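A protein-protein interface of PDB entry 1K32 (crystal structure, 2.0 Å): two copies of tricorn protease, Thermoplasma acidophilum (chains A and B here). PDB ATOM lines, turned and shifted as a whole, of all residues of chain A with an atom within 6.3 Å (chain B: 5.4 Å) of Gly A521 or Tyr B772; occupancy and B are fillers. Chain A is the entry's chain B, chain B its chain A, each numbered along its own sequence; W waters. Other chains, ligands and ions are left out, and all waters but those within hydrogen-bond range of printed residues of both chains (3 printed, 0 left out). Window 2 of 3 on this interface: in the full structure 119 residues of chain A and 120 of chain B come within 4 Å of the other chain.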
ATOM      1  N   PRO A 517       1.637 -11.685   0.359  1.00  0.00           N
ATOM      2  CA  PRO A 517       0.794 -12.891   0.339  1.00  0.00           C
ATOM      3  C   PRO A 517      -0.605 -12.478   0.812  1.00  0.00           C
ATOM      4  O   PRO A 517      -0.733 -11.834   1.846  1.00  0.00           O
ATOM      5  CB  PRO A 517       1.504 -13.820   1.316  1.00  0.00           C
ATOM      6  CG  PRO A 517       2.121 -12.867   2.299  1.00  0.00           C
ATOM      7  CD  PRO A 517       2.683 -11.791   1.394  1.00  0.00           C
ATOM      8  N   ILE A 519      -2.888 -14.338   1.881  1.00  0.00           N
ATOM      9  CA  ILE A 519      -3.287 -15.225   2.968  1.00  0.00           C
ATOM     10  C   ILE A 519      -2.207 -15.104   4.043  1.00  0.00           C
ATOM     11  O   ILE A 519      -1.055 -15.504   3.834  1.00  0.00           O
ATOM     12  CB  ILE A 519      -3.400 -16.700   2.473  1.00  0.00           C
ATOM     13  CG1 ILE A 519      -4.478 -16.783   1.380  1.00  0.00           C
ATOM     14  CG2 ILE A 519      -3.723 -17.631   3.650  1.00  0.00           C
ATOM     15  CD1 ILE A 519      -4.460 -18.044   0.552  1.00  0.00           C
ATOM     16  N   PRO A 520      -2.569 -14.542   5.205  1.00  0.00           N
ATOM     17  CA  PRO A 520      -1.660 -14.341   6.341  1.00  0.00           C
ATOM     18  C   PRO A 520      -1.047 -15.658   6.803  1.00  0.00           C
ATOM     19  O   PRO A 520      -1.751 -16.655   6.916  1.00  0.00           O
ATOM     20  CB  PRO A 520      -2.564 -13.746   7.421  1.00  0.00           C
ATOM     21  CG  PRO A 520      -3.729 -13.173   6.661  1.00  0.00           C
ATOM     22  CD  PRO A 520      -3.952 -14.192   5.576  1.00  0.00           C
ATOM     23  N   GLY A 521       0.254 -15.654   7.079  1.00  0.00           N
ATOM     24  CA  GLY A 521       0.911 -16.866   7.531  1.00  0.00           C
ATOM     25  C   GLY A 521       1.684 -17.511   6.404  1.00  0.00           C
ATOM     26  O   GLY A 521       2.612 -18.279   6.639  1.00  0.00           O
ATOM     27  N   SER A 522       1.288 -17.201   5.172  1.00  0.00           N
ATOM     28  CA  SER A 522       1.953 -17.724   3.985  1.00  0.00           C
ATOM     29  C   SER A 522       3.178 -16.830   3.756  1.00  0.00           C
ATOM     30  O   SER A 522       3.072 -15.610   3.811  1.00  0.00           O
ATOM     31  CB  SER A 522       0.995 -17.657   2.787  1.00  0.00           C
ATOM     32  OG  SER A 522       1.558 -18.262   1.641  1.00  0.00           O
ATOM     33  N   PRO A 523       4.354 -17.430   3.512  1.00  0.00           N
ATOM     34  CA  PRO A 523       5.574 -16.645   3.294  1.00  0.00           C
ATOM     35  C   PRO A 523       5.797 -16.147   1.869  1.00  0.00           C
ATOM     36  O   PRO A 523       5.175 -16.626   0.922  1.00  0.00           O
ATOM     37  CB  PRO A 523       6.668 -17.614   3.721  1.00  0.00           C
ATOM     38  CG  PRO A 523       6.144 -18.906   3.183  1.00  0.00           C
ATOM     39  CD  PRO A 523       4.673 -18.868   3.590  1.00  0.00           C
ATOM     40  N   VAL A 529      10.715 -20.912   0.910  1.00  0.00           N
ATOM     41  CA  VAL A 529      10.571 -21.588   2.189  1.00  0.00           C
ATOM     42  C   VAL A 529      10.011 -22.981   1.897  1.00  0.00           C
ATOM     43  O   VAL A 529       9.015 -23.119   1.193  1.00  0.00           O
ATOM     44  CB  VAL A 529       9.617 -20.807   3.111  1.00  0.00           C
ATOM     45  CG1 VAL A 529       9.333 -21.607   4.374  1.00  0.00           C
ATOM     46  CG2 VAL A 529      10.247 -19.455   3.463  1.00  0.00           C
ATOM     47  N   MET A 533       7.945 -27.076   5.869  1.00  0.00           N
ATOM     48  CA  MET A 533       8.339 -26.278   7.025  1.00  0.00           C
ATOM     49  C   MET A 533       7.437 -25.075   7.184  1.00  0.00           C
ATOM     50  O   MET A 533       7.730 -24.150   7.939  1.00  0.00           O
ATOM     51  CB  MET A 533       9.785 -25.822   6.876  1.00  0.00           C
ATOM     52  CG  MET A 533      10.779 -26.959   6.972  1.00  0.00           C
ATOM     53  SD  MET A 533      12.452 -26.389   6.763  1.00  0.00           S
ATOM     54  CE  MET A 533      13.236 -27.866   6.104  1.00  0.00           C
ATOM     55  N   THR A 534       6.336 -25.090   6.449  1.00  0.00           N
ATOM     56  CA  THR A 534       5.379 -24.003   6.507  1.00  0.00           C
ATOM     57  C   THR A 534       4.010 -24.576   6.800  1.00  0.00           C
ATOM     58  O   THR A 534       3.603 -25.572   6.201  1.00  0.00           O
ATOM     59  CB  THR A 534       5.291 -23.242   5.170  1.00  0.00           C
ATOM     60  OG1 THR A 534       6.599 -22.839   4.760  1.00  0.00           O
ATOM     61  CG2 THR A 534       4.420 -22.005   5.323  1.00  0.00           C
ATOM     62  N   SER A 535       3.307 -23.957   7.738  1.00  0.00           N
ATOM     63  CA  SER A 535       1.963 -24.395   8.065  1.00  0.00           C
ATOM     64  C   SER A 535       1.060 -23.668   7.080  1.00  0.00           C
ATOM     65  O   SER A 535       0.713 -22.509   7.294  1.00  0.00           O
ATOM     66  CB  SER A 535       1.609 -24.022   9.507  1.00  0.00           C
ATOM     67  OG  SER A 535       1.882 -22.660   9.772  1.00  0.00           O
ATOM     68  N   ALA A 537      -2.494 -23.507   4.453  1.00  0.00           N
ATOM     69  CA  ALA A 537      -3.907 -23.250   4.708  1.00  0.00           C
ATOM     70  C   ALA A 537      -4.124 -21.767   4.961  1.00  0.00           C
ATOM     71  O   ALA A 537      -3.267 -20.939   4.643  1.00  0.00           O
ATOM     72  CB  ALA A 537      -4.394 -24.070   5.906  1.00  0.00           C
ATOM     73  N   LYS A 547       1.870  -4.703   6.459  1.00  0.00           N
ATOM     74  CA  LYS A 547       2.744  -5.223   7.503  1.00  0.00           C
ATOM     75  C   LYS A 547       3.406  -6.526   7.069  1.00  0.00           C
ATOM     76  O   LYS A 547       4.489  -6.869   7.541  1.00  0.00           O
ATOM     77  CB  LYS A 547       1.950  -5.454   8.800  1.00  0.00           C
ATOM     78  CG  LYS A 547       1.390  -4.172   9.416  1.00  0.00           C
ATOM     79  CD  LYS A 547       0.747  -4.415  10.777  1.00  0.00           C
ATOM     80  CE  LYS A 547       0.300  -3.103  11.406  1.00  0.00           C
ATOM     81  NZ  LYS A 547      -0.245  -3.262  12.782  1.00  0.00           N
ATOM     82  N   ARG A 548       2.746  -7.230   6.160  1.00  0.00           N
ATOM     83  CA  ARG A 548       3.209  -8.513   5.640  1.00  0.00           C
ATOM     84  C   ARG A 548       4.105  -8.391   4.415  1.00  0.00           C
ATOM     85  O   ARG A 548       4.683  -9.392   3.982  1.00  0.00           O
ATOM     86  CB  ARG A 548       2.019  -9.389   5.216  1.00  0.00           C
ATOM     87  CG  ARG A 548       1.073  -9.817   6.291  1.00  0.00           C
ATOM     88  CD  ARG A 548       0.369 -11.125   5.883  1.00  0.00           C
ATOM     89  NE  ARG A 548      -0.574 -11.006   4.762  1.00  0.00           N
ATOM     90  CZ  ARG A 548      -1.792 -10.472   4.853  1.00  0.00           C
ATOM     91  NH1 ARG A 548      -2.574 -10.417   3.785  1.00  0.00           N
ATOM     92  NH2 ARG A 548      -2.233  -9.980   6.005  1.00  0.00           N
ATOM     93  N   PRO B 768      11.421  -9.638  11.267  1.00  0.00           N
ATOM     94  CA  PRO B 768      11.018 -10.571  10.211  1.00  0.00           C
ATOM     95  C   PRO B 768       9.772 -11.394  10.539  1.00  0.00           C
ATOM     96  O   PRO B 768       9.239 -12.076   9.669  1.00  0.00           O
ATOM     97  CB  PRO B 768      12.262 -11.429  10.013  1.00  0.00           C
ATOM     98  CG  PRO B 768      12.918 -11.388  11.354  1.00  0.00           C
ATOM     99  CD  PRO B 768      12.781  -9.937  11.739  1.00  0.00           C
ATOM    100  N   ILE B 769       9.302 -11.318  11.782  1.00  0.00           N
ATOM    101  CA  ILE B 769       8.102 -12.064  12.183  1.00  0.00           C
ATOM    102  C   ILE B 769       6.851 -11.422  11.606  1.00  0.00           C
ATOM    103  O   ILE B 769       5.843 -12.102  11.381  1.00  0.00           O
ATOM    104  CB  ILE B 769       7.976 -12.154  13.729  1.00  0.00           C
ATOM    105  CG1 ILE B 769       9.009 -13.141  14.261  1.00  0.00           C
ATOM    106  CG2 ILE B 769       6.585 -12.627  14.134  1.00  0.00           C
ATOM    107  CD1 ILE B 769       9.184 -13.099  15.744  1.00  0.00           C
ATOM    108  N   PHE B 770       6.916 -10.115  11.355  1.00  0.00           N
ATOM    109  CA  PHE B 770       5.776  -9.402  10.789  1.00  0.00           C
ATOM    110  C   PHE B 770       5.375  -9.936   9.401  1.00  0.00           C
ATOM    111  O   PHE B 770       4.225  -9.787   8.975  1.00  0.00           O
ATOM    112  CB  PHE B 770       6.070  -7.901  10.680  1.00  0.00           C
ATOM    113  CG  PHE B 770       5.964  -7.153  11.979  1.00  0.00           C
ATOM    114  CD1 PHE B 770       7.105  -6.738  12.649  1.00  0.00           C
ATOM    115  CD2 PHE B 770       4.722  -6.814  12.501  1.00  0.00           C
ATOM    116  CE1 PHE B 770       7.012  -5.991  13.817  1.00  0.00           C
ATOM    117  CE2 PHE B 770       4.623  -6.065  13.673  1.00  0.00           C
ATOM    118  CZ  PHE B 770       5.765  -5.654  14.327  1.00  0.00           C
ATOM    119  N   GLU B 771       6.314 -10.555   8.698  1.00  0.00           N
ATOM    120  CA  GLU B 771       6.024 -11.092   7.376  1.00  0.00           C
ATOM    121  C   GLU B 771       5.101 -12.309   7.435  1.00  0.00           C
ATOM    122  O   GLU B 771       4.653 -12.794   6.399  1.00  0.00           O
ATOM    123  CB  GLU B 771       7.318 -11.463   6.649  1.00  0.00           C
ATOM    124  CG  GLU B 771       8.155 -10.259   6.269  1.00  0.00           C
ATOM    125  CD  GLU B 771       9.242 -10.581   5.258  1.00  0.00           C
ATOM    126  OE1 GLU B 771       9.998  -9.655   4.895  1.00  0.00           O
ATOM    127  OE2 GLU B 771       9.344 -11.748   4.821  1.00  0.00           O
ATOM    128  N   TYR B 772       4.837 -12.802   8.642  1.00  0.00           N
ATOM    129  CA  TYR B 772       3.946 -13.943   8.818  1.00  0.00           C
ATOM    130  C   TYR B 772       2.563 -13.502   9.261  1.00  0.00           C
ATOM    131  O   TYR B 772       1.719 -14.325   9.600  1.00  0.00           O
ATOM    132  CB  TYR B 772       4.520 -14.945   9.818  1.00  0.00           C
ATOM    133  CG  TYR B 772       5.541 -15.863   9.197  1.00  0.00           C
ATOM    134  CD1 TYR B 772       6.905 -15.577   9.260  1.00  0.00           C
ATOM    135  CD2 TYR B 772       5.138 -16.992   8.494  1.00  0.00           C
ATOM    136  CE1 TYR B 772       7.836 -16.392   8.634  1.00  0.00           C
ATOM    137  CE2 TYR B 772       6.054 -17.814   7.867  1.00  0.00           C
ATOM    138  CZ  TYR B 772       7.403 -17.512   7.940  1.00  0.00           C
ATOM    139  OH  TYR B 772       8.310 -18.346   7.336  1.00  0.00           O
ATOM    140  N   GLY B 773       2.349 -12.191   9.281  1.00  0.00           N
ATOM    141  CA  GLY B 773       1.048 -11.656   9.631  1.00  0.00           C
ATOM    142  C   GLY B 773       0.719 -11.369  11.078  1.00  0.00           C
ATOM    143  O   GLY B 773      -0.447 -11.170  11.401  1.00  0.00           O
ATOM    144  N   ILE B 774       1.706 -11.355  11.962  1.00  0.00           N
ATOM    145  CA  ILE B 774       1.398 -11.051  13.355  1.00  0.00           C
ATOM    146  C   ILE B 774       2.453 -10.187  14.006  1.00  0.00           C
ATOM    147  O   ILE B 774       3.601 -10.143  13.571  1.00  0.00           O
ATOM    148  CB  ILE B 774       1.242 -12.322  14.233  1.00  0.00           C
ATOM    149  CG1 ILE B 774       2.578 -13.054  14.334  1.00  0.00           C
ATOM    150  CG2 ILE B 774       0.156 -13.237  13.661  1.00  0.00           C
ATOM    151  CD1 ILE B 774       2.568 -14.202  15.322  1.00  0.00           C
ATOM    152  N   LEU B 821       6.939 -20.666  13.305  1.00  0.00           N
ATOM    153  CA  LEU B 821       7.446 -19.986  12.102  1.00  0.00           C
ATOM    154  C   LEU B 821       8.938 -20.105  11.763  1.00  0.00           C
ATOM    155  O   LEU B 821       9.779 -20.147  12.658  1.00  0.00           O
ATOM    156  CB  LEU B 821       7.118 -18.504  12.239  1.00  0.00           C
ATOM    157  CG  LEU B 821       5.788 -18.207  12.931  1.00  0.00           C
ATOM    158  CD1 LEU B 821       5.783 -16.794  13.455  1.00  0.00           C
ATOM    159  CD2 LEU B 821       4.644 -18.450  11.954  1.00  0.00           C
ATOM    160  N   MET B 822       9.260 -20.144  10.468  1.00  0.00           N
ATOM    161  CA  MET B 822      10.660 -20.212  10.040  1.00  0.00           C
ATOM    162  C   MET B 822      11.084 -18.752   9.907  1.00  0.00           C
ATOM    163  O   MET B 822      10.722 -18.075   8.953  1.00  0.00           O
ATOM    164  CB  MET B 822      10.809 -20.938   8.694  1.00  0.00           C
ATOM    165  CG  MET B 822      10.550 -22.460   8.749  1.00  0.00           C
ATOM    166  SD  MET B 822      11.605 -23.400   9.920  1.00  0.00           S
ATOM    167  CE  MET B 822      13.247 -22.968   9.339  1.00  0.00           C
ATOM    168  N   ILE B 823      11.838 -18.273  10.888  1.00  0.00           N
ATOM    169  CA  ILE B 823      12.252 -16.879  10.905  1.00  0.00           C
ATOM    170  C   ILE B 823      13.695 -16.631  10.501  1.00  0.00           C
ATOM    171  O   ILE B 823      14.601 -17.351  10.894  1.00  0.00           O
ATOM    172  CB  ILE B 823      12.052 -16.265  12.315  1.00  0.00           C
ATOM    173  CG1 ILE B 823      10.612 -16.465  12.777  1.00  0.00           C
ATOM    174  CG2 ILE B 823      12.358 -14.782  12.283  1.00  0.00           C
ATOM    175  CD1 ILE B 823       9.600 -15.773  11.900  1.00  0.00           C
HETATM  176  O   HOH W   1       2.344 -13.726   5.855  1.00  0.00           O
HETATM  177  O   HOH W   2       7.241 -21.087   8.457  1.00  0.00           O
HETATM  178  O   HOH W   3       5.429 -12.029   3.589  1.00  0.00           O
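The side-chain hydroxyl (OH) of Tyr B772 sits at hydrogen-bond distance from the backbone carbonyl oxygen (O) of Met B822, 2.9 Å away.
The backbone carbonyl oxygen of Pro A517 is in hydrogen-bond range of the guanidinium group of Arg A548.
Printed residues of chain B within 4 Å of Gly A521: Tyr B772.
Tyr B772 touches just one residue of chain A: Gly A521.
Printed residues of chain A within 4 Å of Met B822: Met A533.
Of the printed residues of chain B, Met A533 touches Met B822 (3.4 Å).
The nearest printed residue of chain A that does not touch Met B822 is Val A529 (4.6 Å).
Water W1 lies within hydrogen-bond range of O of Glu B771 (2.5 Å), O of Ser A522 (2.9 Å) and N of Gly A521 (3.1 Å).
Water W3 lies within hydrogen-bond range of the backbone carbonyl oxygen (O) of Arg A548 and the backbone carbonyl oxygen (O) of Glu B771.
Water W2 lies within hydrogen-bond range of the backbone NH of Met B822, the backbone carbonyl oxygen of Met A533 and the side-chain hydroxyl of Tyr B772.
The backbone carbonyl oxygen (O) of Lys A547 lies close to the backbone carbonyl oxygen (O) of Phe B770 (3.3 Å).
N of Gly A521 is in hydrogen-bond range of O of Tyr B772 (3.2 Å).
Among the printed residues, merely in contact across the chains: Met A533 with Met B822 (3.4 Å), Arg A548 with Phe B770 (3.7 Å) and Arg A548 with Gly B773 (3.8 Å).
Printed residues of chain B that touch a printed residue of chain A: Phe B770, Tyr B772, Gly B773 and Met B822.
Hydrophobic or aromatic side chains of chain B that line the printed part of chain A: Phe B770, Tyr B772 and Met B822.
Of the 13 printed residues of chain A, 4 touch a printed residue of chain B.
Printed residues of chain A that touch a printed residue of chain B: Gly A521, Met A533, Lys A547 and Arg A548.
Among the printed residues, 5 pairs touch across the chains.
Among the printed residues, no Asp or Glu carboxylate lies within 4 Å of a Lys or Arg side-chain nitrogen of the other chain.
No position is printed for both chains.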
